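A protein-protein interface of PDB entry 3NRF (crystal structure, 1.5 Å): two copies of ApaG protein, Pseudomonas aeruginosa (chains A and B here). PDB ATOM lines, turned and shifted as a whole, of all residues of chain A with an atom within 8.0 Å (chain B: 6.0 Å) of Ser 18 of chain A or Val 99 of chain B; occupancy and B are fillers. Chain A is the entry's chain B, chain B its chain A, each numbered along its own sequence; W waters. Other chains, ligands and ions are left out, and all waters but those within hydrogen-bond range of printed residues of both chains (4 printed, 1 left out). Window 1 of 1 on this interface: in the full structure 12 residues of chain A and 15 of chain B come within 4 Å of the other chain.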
ATOM      1  N   ASP A  15      -2.091   0.825  12.418  1.00  0.00           N
ATOM      2  CA  ASP A  15      -2.168  -0.583  12.103  1.00  0.00           C
ATOM      3  C   ASP A  15      -0.857  -1.395  12.371  1.00  0.00           C
ATOM      4  O   ASP A  15       0.262  -0.866  12.314  1.00  0.00           O
ATOM      5  CB  ASP A  15      -2.490  -0.775  10.604  1.00  0.00           C
ATOM      6  CG  ASP A  15      -3.873  -0.300  10.202  1.00  0.00           C
ATOM      7  OD1 ASP A  15      -4.735  -0.091  11.077  1.00  0.00           O
ATOM      8  OD2 ASP A  15      -4.074  -0.172   8.967  1.00  0.00           O
ATOM      9  N   LYS A  16      -1.063  -2.690  12.634  1.00  0.00           N
ATOM     10  CA  LYS A  16      -0.019  -3.690  12.890  1.00  0.00           C
ATOM     11  C   LYS A  16       0.105  -4.646  11.702  1.00  0.00           C
ATOM     12  O   LYS A  16      -0.903  -5.279  11.268  1.00  0.00           O
ATOM     13  CB  LYS A  16      -0.347  -4.515  14.129  1.00  0.00           C
ATOM     14  CG  LYS A  16      -0.419  -3.707  15.421  1.00  0.00           C
ATOM     15  CD  LYS A  16      -0.769  -4.564  16.642  1.00  0.00           C
ATOM     16  CE  LYS A  16      -1.337  -3.705  17.809  1.00  0.00           C
ATOM     17  NZ  LYS A  16      -0.494  -2.508  18.175  1.00  0.00           N
ATOM     18  N   GLY A  17       1.351  -4.836  11.249  1.00  0.00           N
ATOM     19  CA  GLY A  17       1.595  -5.633  10.086  1.00  0.00           C
ATOM     20  C   GLY A  17       2.879  -6.415  10.169  1.00  0.00           C
ATOM     21  O   GLY A  17       3.520  -6.532  11.206  1.00  0.00           O
ATOM     22  N   SER A  18       3.200  -6.981   9.024  1.00  0.00           N
ATOM     23  CA  SER A  18       4.433  -7.728   8.904  1.00  0.00           C
ATOM     24  C   SER A  18       4.948  -7.696   7.483  1.00  0.00           C
ATOM     25  O   SER A  18       4.186  -7.514   6.519  1.00  0.00           O
ATOM     26  CB  SER A  18       4.285  -9.187   9.392  1.00  0.00           C
ATOM     27  OG  SER A  18       3.409  -9.939   8.571  1.00  0.00           O
ATOM     28  N   VAL A  19       6.264  -7.934   7.333  1.00  0.00           N
ATOM     29  CA  VAL A  19       6.904  -8.042   6.050  1.00  0.00           C
ATOM     30  C   VAL A  19       7.884  -9.212   6.112  1.00  0.00           C
ATOM     31  O   VAL A  19       8.623  -9.330   7.067  1.00  0.00           O
ATOM     32  CB  VAL A  19       7.754  -6.747   5.689  1.00  0.00           C
ATOM     33  CG1 VAL A  19       8.473  -6.861   4.326  1.00  0.00           C
ATOM     34  CG2 VAL A  19       6.845  -5.457   5.773  1.00  0.00           C
ATOM     35  N   SER A  20       7.865 -10.027   5.090  1.00  0.00           N
ATOM     36  CA  SER A  20       8.755 -11.204   4.970  1.00  0.00           C
ATOM     37  C   SER A  20       9.306 -11.331   3.569  1.00  0.00           C
ATOM     38  O   SER A  20       8.568 -11.307   2.593  1.00  0.00           O
ATOM     39  CB  SER A  20       7.984 -12.459   5.296  1.00  0.00           C
ATOM     40  OG  SER A  20       8.812 -13.594   5.219  1.00  0.00           O
ATOM     41  N   VAL A  21      10.628 -11.470   3.464  1.00  0.00           N
ATOM     42  CA  VAL A  21      11.244 -11.700   2.175  1.00  0.00           C
ATOM     43  C   VAL A  21      12.469 -12.590   2.409  1.00  0.00           C
ATOM     44  O   VAL A  21      13.379 -12.257   3.130  1.00  0.00           O
ATOM     45  CB  VAL A  21      11.530 -10.400   1.390  1.00  0.00           C
ATOM     46  CG1 VAL A  21      12.390  -9.456   2.209  1.00  0.00           C
ATOM     47  CG2 VAL A  21      12.135 -10.752   0.038  1.00  0.00           C
ATOM     48  N   LYS A  24      14.324 -12.992   5.830  1.00  0.00           N
ATOM     49  CA  LYS A  24      14.165 -11.809   6.632  1.00  0.00           C
ATOM     50  C   LYS A  24      12.704 -11.545   6.933  1.00  0.00           C
ATOM     51  O   LYS A  24      11.898 -11.422   5.988  1.00  0.00           O
ATOM     52  CB  LYS A  24      14.757 -10.641   5.840  1.00  0.00           C
ATOM     53  CG  LYS A  24      14.717  -9.296   6.517  1.00  0.00           C
ATOM     54  CD  LYS A  24      15.399  -8.239   5.616  1.00  0.00           C
ATOM     55  CE  LYS A  24      15.323  -6.827   6.220  1.00  0.00           C
ATOM     56  NZ  LYS A  24      16.016  -6.741   7.548  1.00  0.00           N
ATOM     57  N   HIS A  25      12.401 -11.446   8.222  1.00  0.00           N
ATOM     58  CA  HIS A  25      11.032 -11.274   8.674  1.00  0.00           C
ATOM     59  C   HIS A  25      11.000 -10.119   9.663  1.00  0.00           C
ATOM     60  O   HIS A  25      11.878 -10.013  10.534  1.00  0.00           O
ATOM     61  CB  HIS A  25      10.554 -12.533   9.410  1.00  0.00           C
ATOM     62  CG  HIS A  25      10.853 -13.798   8.687  1.00  0.00           C
ATOM     63  ND1 HIS A  25      10.350 -14.073   7.436  1.00  0.00           N
ATOM     64  CD2 HIS A  25      11.624 -14.862   9.018  1.00  0.00           C
ATOM     65  CE1 HIS A  25      10.834 -15.228   7.002  1.00  0.00           C
ATOM     66  NE2 HIS A  25      11.571 -15.753   7.970  1.00  0.00           N
ATOM     67  N   PHE A  26       9.977  -9.262   9.579  1.00  0.00           N
ATOM     68  CA  PHE A  26       9.808  -8.257  10.613  1.00  0.00           C
ATOM     69  C   PHE A  26       8.347  -7.854  10.787  1.00  0.00           C
ATOM     70  O   PHE A  26       7.541  -8.031   9.902  1.00  0.00           O
ATOM     71  CB  PHE A  26      10.755  -7.065  10.444  1.00  0.00           C
ATOM     72  CG  PHE A  26      10.578  -6.262   9.215  1.00  0.00           C
ATOM     73  CD1 PHE A  26       9.709  -5.189   9.173  1.00  0.00           C
ATOM     74  CD2 PHE A  26      11.417  -6.470   8.099  1.00  0.00           C
ATOM     75  CE1 PHE A  26       9.600  -4.404   8.022  1.00  0.00           C
ATOM     76  CE2 PHE A  26      11.313  -5.676   6.970  1.00  0.00           C
ATOM     77  CZ  PHE A  26      10.388  -4.645   6.919  1.00  0.00           C
ATOM     78  N   ARG A  27       8.047  -7.413  11.996  1.00  0.00           N
ATOM     79  CA  ARG A  27       6.727  -6.908  12.369  1.00  0.00           C
ATOM     80  C   ARG A  27       6.761  -5.400  12.274  1.00  0.00           C
ATOM     81  O   ARG A  27       7.842  -4.785  12.492  1.00  0.00           O
ATOM     82  CB  ARG A  27       6.359  -7.331  13.781  1.00  0.00           C
ATOM     83  CG  ARG A  27       5.880  -8.742  13.909  1.00  0.00           C
ATOM     84  CD  ARG A  27       6.960  -9.809  13.671  1.00  0.00           C
ATOM     85  NE  ARG A  27       6.430 -11.140  13.970  1.00  0.00           N
ATOM     86  CZ  ARG A  27       7.141 -12.267  13.909  1.00  0.00           C
ATOM     87  NH1 ARG A  27       8.425 -12.196  13.564  1.00  0.00           N
ATOM     88  NH2 ARG A  27       6.558 -13.415  14.188  1.00  0.00           N
ATOM     89  N   THR A  28       5.634  -4.798  11.893  1.00  0.00           N
ATOM     90  CA  THR A  28       5.555  -3.352  11.726  1.00  0.00           C
ATOM     91  C   THR A  28       4.462  -2.746  12.584  1.00  0.00           C
ATOM     92  O   THR A  28       3.440  -3.385  12.834  1.00  0.00           O
ATOM     93  CB  THR A  28       5.292  -2.940  10.275  1.00  0.00           C
ATOM     94  OG1 THR A  28       4.048  -3.518   9.841  1.00  0.00           O
ATOM     95  CG2 THR A  28       6.443  -3.413   9.361  1.00  0.00           C
ATOM     96  N   GLN A  29       4.726  -1.546  13.095  1.00  0.00           N
ATOM     97  CA  GLN A  29       3.731  -0.771  13.850  1.00  0.00           C
ATOM     98  C   GLN A  29       3.690   0.634  13.251  1.00  0.00           C
ATOM     99  O   GLN A  29       4.686   1.356  13.266  1.00  0.00           O
ATOM    100  CB  GLN A  29       4.083  -0.674  15.340  1.00  0.00           C
ATOM    101  CG  GLN A  29       3.121   0.224  16.125  1.00  0.00           C
ATOM    102  CD  GLN A  29       1.712  -0.326  16.178  1.00  0.00           C
ATOM    103  OE1 GLN A  29       1.471  -1.403  16.726  1.00  0.00           O
ATOM    104  NE2 GLN A  29       0.772   0.437  15.595  1.00  0.00           N
ATOM    105  N   ILE A  85       6.238   4.329  10.009  1.00  0.00           N
ATOM    106  CA  ILE A  85       6.114   2.911  10.332  1.00  0.00           C
ATOM    107  C   ILE A  85       7.436   2.379  10.877  1.00  0.00           C
ATOM    108  O   ILE A  85       8.472   2.527  10.205  1.00  0.00           O
ATOM    109  CB  ILE A  85       5.686   2.047   9.098  1.00  0.00           C
ATOM    110  CG1 ILE A  85       4.359   2.513   8.540  1.00  0.00           C
ATOM    111  CG2 ILE A  85       5.560   0.616   9.487  1.00  0.00           C
ATOM    112  CD1 ILE A  85       3.909   1.695   7.298  1.00  0.00           C
ATOM    113  N   SER A  88      10.394  -4.247  14.144  1.00  0.00           N
ATOM    114  CA  SER A  88      11.196  -5.150  14.972  1.00  0.00           C
ATOM    115  C   SER A  88      11.136  -6.532  14.356  1.00  0.00           C
ATOM    116  O   SER A  88      10.178  -6.840  13.648  1.00  0.00           O
ATOM    117  CB  SER A  88      10.727  -5.217  16.415  1.00  0.00           C
ATOM    118  OG  SER A  88       9.379  -5.637  16.545  1.00  0.00           O
ATOM    119  N   GLU A  89      12.132  -7.378  14.620  1.00  0.00           N
ATOM    120  CA  GLU A  89      12.102  -8.726  14.033  1.00  0.00           C
ATOM    121  C   GLU A  89      11.041  -9.574  14.673  1.00  0.00           C
ATOM    122  O   GLU A  89      10.416 -10.402  13.979  1.00  0.00           O
ATOM    123  CB  GLU A  89      13.427  -9.450  14.253  1.00  0.00           C
ATOM    124  CG  GLU A  89      14.553  -8.703  13.595  1.00  0.00           C
ATOM    125  CD  GLU A  89      15.298  -7.761  14.547  1.00  0.00           C
ATOM    126  OE1 GLU A  89      14.698  -7.142  15.461  1.00  0.00           O
ATOM    127  OE2 GLU A  89      16.560  -7.683  14.417  1.00  0.00           O
ATOM    128  N   ASP A  91       7.919  -9.392  18.070  1.00  0.00           N
ATOM    129  CA  ASP A  91       6.755  -8.599  18.363  1.00  0.00           C
ATOM    130  C   ASP A  91       7.069  -7.344  19.186  1.00  0.00           C
ATOM    131  O   ASP A  91       6.149  -6.598  19.503  1.00  0.00           O
ATOM    132  CB  ASP A  91       5.703  -9.401  19.128  1.00  0.00           C
ATOM    133  CG  ASP A  91       4.947 -10.363  18.258  1.00  0.00           C
ATOM    134  OD1 ASP A  91       5.236 -10.458  17.045  1.00  0.00           O
ATOM    135  OD2 ASP A  91       4.019 -10.975  18.825  1.00  0.00           O
ATOM    136  N   TYR A  94       5.393  -3.855  18.917  1.00  0.00           N
ATOM    137  CA  TYR A  94       4.016  -3.673  19.361  1.00  0.00           C
ATOM    138  C   TYR A  94       3.915  -3.064  20.713  1.00  0.00           C
ATOM    139  O   TYR A  94       2.827  -2.502  21.066  1.00  0.00           O
ATOM    140  CB  TYR A  94       3.285  -5.010  19.279  1.00  0.00           C
ATOM    141  CG  TYR A  94       3.226  -5.482  17.849  1.00  0.00           C
ATOM    142  CD1 TYR A  94       3.059  -4.597  16.777  1.00  0.00           C
ATOM    143  CD2 TYR A  94       3.285  -6.831  17.533  1.00  0.00           C
ATOM    144  CE1 TYR A  94       3.039  -5.009  15.503  1.00  0.00           C
ATOM    145  CE2 TYR A  94       3.195  -7.266  16.209  1.00  0.00           C
ATOM    146  CZ  TYR A  94       3.078  -6.345  15.181  1.00  0.00           C
ATOM    147  OH  TYR A  94       2.995  -6.856  13.881  1.00  0.00           O
ATOM    148  N   VAL B   9       6.264 -10.771   1.040  1.00  0.00           N
ATOM    149  CA  VAL B   9       4.965 -11.034   1.633  1.00  0.00           C
ATOM    150  C   VAL B   9       4.644  -9.937   2.604  1.00  0.00           C
ATOM    151  O   VAL B   9       5.308  -9.806   3.630  1.00  0.00           O
ATOM    152  CB  VAL B   9       4.919 -12.420   2.388  1.00  0.00           C
ATOM    153  CG1 VAL B   9       3.537 -12.732   2.961  1.00  0.00           C
ATOM    154  CG2 VAL B   9       5.502 -13.532   1.485  1.00  0.00           C
ATOM    155  N   PHE B  10       3.587  -9.157   2.317  1.00  0.00           N
ATOM    156  CA  PHE B  10       3.123  -8.094   3.202  1.00  0.00           C
ATOM    157  C   PHE B  10       1.819  -8.529   3.827  1.00  0.00           C
ATOM    158  O   PHE B  10       0.985  -9.083   3.128  1.00  0.00           O
ATOM    159  CB  PHE B  10       2.857  -6.812   2.381  1.00  0.00           C
ATOM    160  CG  PHE B  10       4.093  -6.248   1.742  1.00  0.00           C
ATOM    161  CD1 PHE B  10       4.541  -6.677   0.459  1.00  0.00           C
ATOM    162  CD2 PHE B  10       4.846  -5.308   2.404  1.00  0.00           C
ATOM    163  CE1 PHE B  10       5.733  -6.142  -0.128  1.00  0.00           C
ATOM    164  CE2 PHE B  10       6.052  -4.797   1.832  1.00  0.00           C
ATOM    165  CZ  PHE B  10       6.478  -5.204   0.583  1.00  0.00           C
ATOM    166  N   ALA B  11       1.643  -8.327   5.126  1.00  0.00           N
ATOM    167  CA  ALA B  11       0.414  -8.761   5.742  1.00  0.00           C
ATOM    168  C   ALA B  11      -0.048  -7.814   6.821  1.00  0.00           C
ATOM    169  O   ALA B  11       0.748  -7.110   7.415  1.00  0.00           O
ATOM    170  CB  ALA B  11       0.606 -10.181   6.333  1.00  0.00           C
ATOM    171  N   ARG B  12      -1.356  -7.789   7.022  1.00  0.00           N
ATOM    172  CA  ARG B  12      -1.944  -6.961   8.083  1.00  0.00           C
ATOM    173  C   ARG B  12      -2.865  -7.857   8.863  1.00  0.00           C
ATOM    174  O   ARG B  12      -3.675  -8.548   8.321  1.00  0.00           O
ATOM    175  CB  ARG B  12      -2.710  -5.772   7.501  1.00  0.00           C
ATOM    176  CG  ARG B  12      -3.339  -4.854   8.552  1.00  0.00           C
ATOM    177  CD  ARG B  12      -4.187  -3.831   7.864  1.00  0.00           C
ATOM    178  NE  ARG B  12      -5.197  -4.497   7.044  1.00  0.00           N
ATOM    179  CZ  ARG B  12      -6.029  -3.876   6.213  1.00  0.00           C
ATOM    180  NH1 ARG B  12      -5.982  -2.559   6.078  1.00  0.00           N
ATOM    181  NH2 ARG B  12      -6.906  -4.581   5.514  1.00  0.00           N
ATOM    182  N   PHE B  31      -5.595 -12.604   8.019  1.00  0.00           N
ATOM    183  CA  PHE B  31      -4.729 -11.549   7.610  1.00  0.00           C
ATOM    184  C   PHE B  31      -5.088 -11.144   6.183  1.00  0.00           C
ATOM    185  O   PHE B  31      -5.537 -11.988   5.387  1.00  0.00           O
ATOM    186  CB  PHE B  31      -3.249 -11.991   7.522  1.00  0.00           C
ATOM    187  CG  PHE B  31      -2.628 -12.394   8.831  1.00  0.00           C
ATOM    188  CD1 PHE B  31      -2.869 -13.644   9.375  1.00  0.00           C
ATOM    189  CD2 PHE B  31      -1.754 -11.537   9.498  1.00  0.00           C
ATOM    190  CE1 PHE B  31      -2.297 -14.006  10.571  1.00  0.00           C
ATOM    191  CE2 PHE B  31      -1.163 -11.933  10.711  1.00  0.00           C
ATOM    192  CZ  PHE B  31      -1.444 -13.163  11.219  1.00  0.00           C
ATOM    193  N   VAL B  33      -3.229 -10.226   2.891  1.00  0.00           N
ATOM    194  CA  VAL B  33      -1.882 -10.558   2.423  1.00  0.00           C
ATOM    195  C   VAL B  33      -1.685 -10.090   1.025  1.00  0.00           C
ATOM    196  O   VAL B  33      -2.578 -10.309   0.180  1.00  0.00           O
ATOM    197  CB  VAL B  33      -1.672 -12.064   2.444  1.00  0.00           C
ATOM    198  CG1 VAL B  33      -0.304 -12.417   1.877  1.00  0.00           C
ATOM    199  CG2 VAL B  33      -1.818 -12.605   3.841  1.00  0.00           C
ATOM    200  N   LEU B  50       1.731 -20.597   2.189  1.00  0.00           N
ATOM    201  CA  LEU B  50       1.636 -19.503   3.117  1.00  0.00           C
ATOM    202  C   LEU B  50       1.476 -20.060   4.518  1.00  0.00           C
ATOM    203  O   LEU B  50       0.611 -20.938   4.747  1.00  0.00           O
ATOM    204  CB  LEU B  50       0.430 -18.584   2.807  1.00  0.00           C
ATOM    205  CG  LEU B  50       0.567 -17.618   1.641  1.00  0.00           C
ATOM    206  CD1 LEU B  50      -0.802 -16.938   1.316  1.00  0.00           C
ATOM    207  CD2 LEU B  50       1.627 -16.551   1.895  1.00  0.00           C
ATOM    208  N   VAL B  51       2.217 -19.503   5.483  1.00  0.00           N
ATOM    209  CA  VAL B  51       2.130 -19.919   6.856  1.00  0.00           C
ATOM    210  C   VAL B  51       2.144 -18.699   7.752  1.00  0.00           C
ATOM    211  O   VAL B  51       2.820 -17.705   7.449  1.00  0.00           O
ATOM    212  CB  VAL B  51       3.265 -20.911   7.132  1.00  0.00           C
ATOM    213  CG1 VAL B  51       3.643 -21.036   8.622  1.00  0.00           C
ATOM    214  CG2 VAL B  51       2.864 -22.287   6.494  1.00  0.00           C
ATOM    215  N   ALA B  52       1.371 -18.732   8.810  1.00  0.00           N
ATOM    216  CA  ALA B  52       1.348 -17.657   9.813  1.00  0.00           C
ATOM    217  C   ALA B  52       2.225 -18.153  10.969  1.00  0.00           C
ATOM    218  O   ALA B  52       2.288 -19.329  11.250  1.00  0.00           O
ATOM    219  CB  ALA B  52      -0.066 -17.279  10.284  1.00  0.00           C
ATOM    220  N   GLN B  53       2.879 -17.218  11.666  1.00  0.00           N
ATOM    221  CA  GLN B  53       3.829 -17.581  12.693  1.00  0.00           C
ATOM    222  C   GLN B  53       3.823 -16.592  13.853  1.00  0.00           C
ATOM    223  O   GLN B  53       3.728 -15.383  13.643  1.00  0.00           O
ATOM    224  CB  GLN B  53       5.250 -17.636  12.080  1.00  0.00           C
ATOM    225  CG  GLN B  53       6.293 -18.378  12.929  1.00  0.00           C
ATOM    226  CD  GLN B  53       7.724 -18.284  12.374  1.00  0.00           C
ATOM    227  OE1 GLN B  53       7.960 -17.736  11.302  1.00  0.00           O
ATOM    228  NE2 GLN B  53       8.681 -18.800  13.128  1.00  0.00           N
ATOM    229  N   ALA B  84      -6.331 -14.332   3.954  1.00  0.00           N
ATOM    230  CA  ALA B  84      -5.857 -15.678   4.255  1.00  0.00           C
ATOM    231  C   ALA B  84      -6.163 -15.921   5.724  1.00  0.00           C
ATOM    232  O   ALA B  84      -5.896 -15.064   6.561  1.00  0.00           O
ATOM    233  CB  ALA B  84      -4.354 -15.728   4.010  1.00  0.00           C
ATOM    234  N   PHE B  86      -5.820 -18.487   8.955  1.00  0.00           N
ATOM    235  CA  PHE B  86      -4.986 -19.547   9.570  1.00  0.00           C
ATOM    236  C   PHE B  86      -5.736 -20.047  10.805  1.00  0.00           C
ATOM    237  O   PHE B  86      -6.553 -19.335  11.360  1.00  0.00           O
ATOM    238  CB  PHE B  86      -3.583 -19.000   9.887  1.00  0.00           C
ATOM    239  CG  PHE B  86      -2.924 -18.419   8.695  1.00  0.00           C
ATOM    240  CD1 PHE B  86      -3.140 -17.108   8.315  1.00  0.00           C
ATOM    241  CD2 PHE B  86      -2.107 -19.226   7.938  1.00  0.00           C
ATOM    242  CE1 PHE B  86      -2.494 -16.587   7.163  1.00  0.00           C
ATOM    243  CE2 PHE B  86      -1.494 -18.733   6.802  1.00  0.00           C
ATOM    244  CZ  PHE B  86      -1.685 -17.422   6.397  1.00  0.00           C
ATOM    245  N   SER B  97       1.729 -13.281  14.256  1.00  0.00           N
ATOM    246  CA  SER B  97       1.964 -11.905  13.919  1.00  0.00           C
ATOM    247  C   SER B  97       2.705 -11.737  12.592  1.00  0.00           C
ATOM    248  O   SER B  97       3.018 -10.608  12.237  1.00  0.00           O
ATOM    249  CB  SER B  97       2.781 -11.216  14.999  1.00  0.00           C
ATOM    250  OG  SER B  97       4.000 -11.892  15.269  1.00  0.00           O
ATOM    251  N   LEU B  98       3.049 -12.828  11.929  1.00  0.00           N
ATOM    252  CA  LEU B  98       3.780 -12.752  10.664  1.00  0.00           C
ATOM    253  C   LEU B  98       3.161 -13.717   9.685  1.00  0.00           C
ATOM    254  O   LEU B  98       2.736 -14.826  10.094  1.00  0.00           O
ATOM    255  CB  LEU B  98       5.201 -13.211  10.917  1.00  0.00           C
ATOM    256  CG  LEU B  98       6.197 -13.495   9.735  1.00  0.00           C
ATOM    257  CD1 LEU B  98       6.590 -12.149   9.143  1.00  0.00           C
ATOM    258  CD2 LEU B  98       7.414 -14.320  10.189  1.00  0.00           C
ATOM    259  N   VAL B  99       3.167 -13.350   8.407  1.00  0.00           N
ATOM    260  CA  VAL B  99       2.806 -14.275   7.328  1.00  0.00           C
ATOM    261  C   VAL B  99       4.043 -14.416   6.459  1.00  0.00           C
ATOM    262  O   VAL B  99       4.725 -13.411   6.084  1.00  0.00           O
ATOM    263  CB  VAL B  99       1.573 -13.872   6.480  1.00  0.00           C
ATOM    264  CG1 VAL B  99       1.295 -14.924   5.409  1.00  0.00           C
ATOM    265  CG2 VAL B  99       0.306 -13.815   7.401  1.00  0.00           C
ATOM    266  N   ARG B 100       4.442 -15.638   6.176  1.00  0.00           N
ATOM    267  CA  ARG B 100       5.605 -15.902   5.319  1.00  0.00           C
ATOM    268  C   ARG B 100       5.333 -17.007   4.326  1.00  0.00           C
ATOM    269  O   ARG B 100       4.376 -17.740   4.473  1.00  0.00           O
ATOM    270  CB  ARG B 100       6.833 -16.289   6.165  1.00  0.00           C
ATOM    271  CG  ARG B 100       6.695 -17.621   6.923  1.00  0.00           C
ATOM    272  CD  ARG B 100       7.879 -17.827   7.849  1.00  0.00           C
ATOM    273  NE  ARG B 100       7.781 -19.023   8.681  1.00  0.00           N
ATOM    274  CZ  ARG B 100       8.176 -20.231   8.289  1.00  0.00           C
ATOM    275  NH1 ARG B 100       8.637 -20.399   7.068  1.00  0.00           N
ATOM    276  NH2 ARG B 100       8.042 -21.266   9.100  1.00  0.00           N
ATOM    277  N   LEU B 101       6.187 -17.143   3.321  1.00  0.00           N
ATOM    278  CA  LEU B 101       6.097 -18.272   2.408  1.00  0.00           C
ATOM    279  C   LEU B 101       7.123 -19.305   2.925  1.00  0.00           C
ATOM    280  O   LEU B 101       8.281 -18.979   3.163  1.00  0.00           O
ATOM    281  CB  LEU B 101       6.513 -17.851   0.989  1.00  0.00           C
ATOM    282  CG  LEU B 101       5.405 -17.108   0.252  1.00  0.00           C
ATOM    283  CD1 LEU B 101       5.920 -16.318  -0.975  1.00  0.00           C
ATOM    284  CD2 LEU B 101       4.351 -18.100  -0.209  1.00  0.00           C
HETATM  285  O   HOH W   1       0.827  -9.302  10.128  1.00  0.00           O
HETATM  286  O   HOH W   2       4.297 -10.730   6.136  1.00  0.00           O
HETATM  287  O   HOH W   3       8.496 -15.330   3.112  1.00  0.00           O
HETATM  288  O   HOH W   4       1.323  -8.558  12.704  1.00  0.00           O
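The backbone carbonyl oxygen of Ser 20 of chain A is in hydrogen-bond range of the backbone NH of Val 9 of chain B, 2.8 Å away.
The backbone carbonyl oxygen of Ala 11 of chain B sits at hydrogen-bond distance from the backbone NH of Ser 18 of chain A, 2.9 Å away.
O of Gln 53 of chain B is in hydrogen-bond range of NH2 of Arg 27 of chain A, 3.5 Å away.
NE of Arg 27 of chain A sits at hydrogen-bond distance from OG of Ser 97 of chain B, at 2.9 Å.
The side-chain hydroxyl (OG) of Ser 97 of chain B sits at hydrogen-bond distance from the side-chain carboxylate (OD1) of Asp 91 of chain A.
N of Val 99 of chain B sits at hydrogen-bond distance from OG of Ser 18 of chain A (3.4 Å).
Water W4 lies within hydrogen-bond range of OH of Tyr 94 of chain A (2.7 Å), O of Ser 97 of chain B (2.7 Å) and O of Gly 17 of chain A (3.3 Å).
Water W2 lies within hydrogen-bond range of the side-chain hydroxyl (OG) of Ser 18 of chain A (2.7 Å), the backbone carbonyl oxygen (O) of Val 99 of chain B (2.7 Å) and the backbone carbonyl oxygen (O) of Val 9 of chain B (2.9 Å).
Water W3 lies within hydrogen-bond range of OG of Ser 20 of chain A (2.7 Å) and N of Leu 101 of chain B (2.9 Å).
Water W1 lies within hydrogen-bond range of the side-chain hydroxyl of Ser 18 of chain A (3.1 Å), the backbone carbonyl oxygen of Ser 97 of chain B (3.3 Å) and the backbone carbonyl oxygen of Ala 11 of chain B (3.5 Å).
Among the printed residues, pairs that only touch across the chains: Gly 17 of chain A with Ala 11 of chain B, Val 19 of chain A with Val 9 of chain B, Ser 18 of chain A with Ser 97 of chain B, Ser 20 of chain A with Arg 100 of chain B, Ser 20 of chain A with Val 99 of chain B, Ser 18 of chain A with Leu 98 of chain B, Ser 18 of chain A with Phe 10 of chain B, Arg 27 of chain A with Leu 98 of chain B, Lys 16 of chain A with Arg 12 of chain B, His 25 of chain A with Leu 98 of chain B, Asp 15 of chain A with Arg 12 of chain B, Ser 18 of chain A with Val 9 of chain B and Val 19 of chain A with Phe 10 of chain B.
The backbone carbonyl oxygen (O) of Val 51 of chain B is in hydrogen-bond range of the backbone NH (N) of Arg 100 of chain B.
The side-chain hydroxyl (OH) of Tyr 94 of chain A sits at hydrogen-bond distance from the backbone carbonyl oxygen (O) of Gly 17 of chain A, at 2.7 Å.
OG of Ser 20 of chain A is in hydrogen-bond range of ND1 of His 25 of chain A, at 2.7 Å.
The backbone NH (N) of Arg 27 of chain A sits at hydrogen-bond distance from the backbone carbonyl oxygen (O) of Ser 88 of chain A.
The guanidinium group (NH1) of Arg 27 of chain A sits at hydrogen-bond distance from the backbone carbonyl oxygen (O) of Glu 89 of chain A, at 2.7 Å.
The guanidinium group (NE) of Arg 27 of chain A is in salt-bridge range of the side-chain carboxylate (OD1) of Asp 91 of chain A (3.4 Å).
No position is printed for both chains.
Printed residues of chain B that touch a printed residue of chain A: Val 9, Phe 10, Ala 11, Arg 12, Gln 53, Ser 97, Leu 98, Val 99 and Arg 100.
Hydrophobic or aromatic side chains of chain B that line the printed part of chain A: Val 9, Phe 10, Ala 11 and Leu 98.
Of the 18 printed residues of chain A, 9 touch a printed residue of chain B.
Among the printed residues, 19 pairs touch across the chains.
Of the printed residues of chain B, Lys 16 of chain A touches Arg 12.
Printed residues of chain B within 4 Å of Ser 18 of chain A: Val 9, Phe 10, Ala 11, Ser 97, Leu 98 and Val 99.
Of the printed residues of chain B, His 25 of chain A touches Leu 98 (3.7 Å).
Of the printed residues of chain A, Val 9 of chain B touches Ser 18 (3.9 Å), Val 19 (3.4 Å) and Ser 20 (2.8 Å).
Of the printed residues of chain A, Arg 12 of chain B touches Asp 15 and Lys 16.
Of chain A, only Ser 18 (3.4 Å) and Ser 20 (3.5 Å) come within 4 Å of Val 99 of chain B.
The nearest residue of chain A that does not touch Val 99 of chain B is Val 19 of chain A (5.3 Å).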
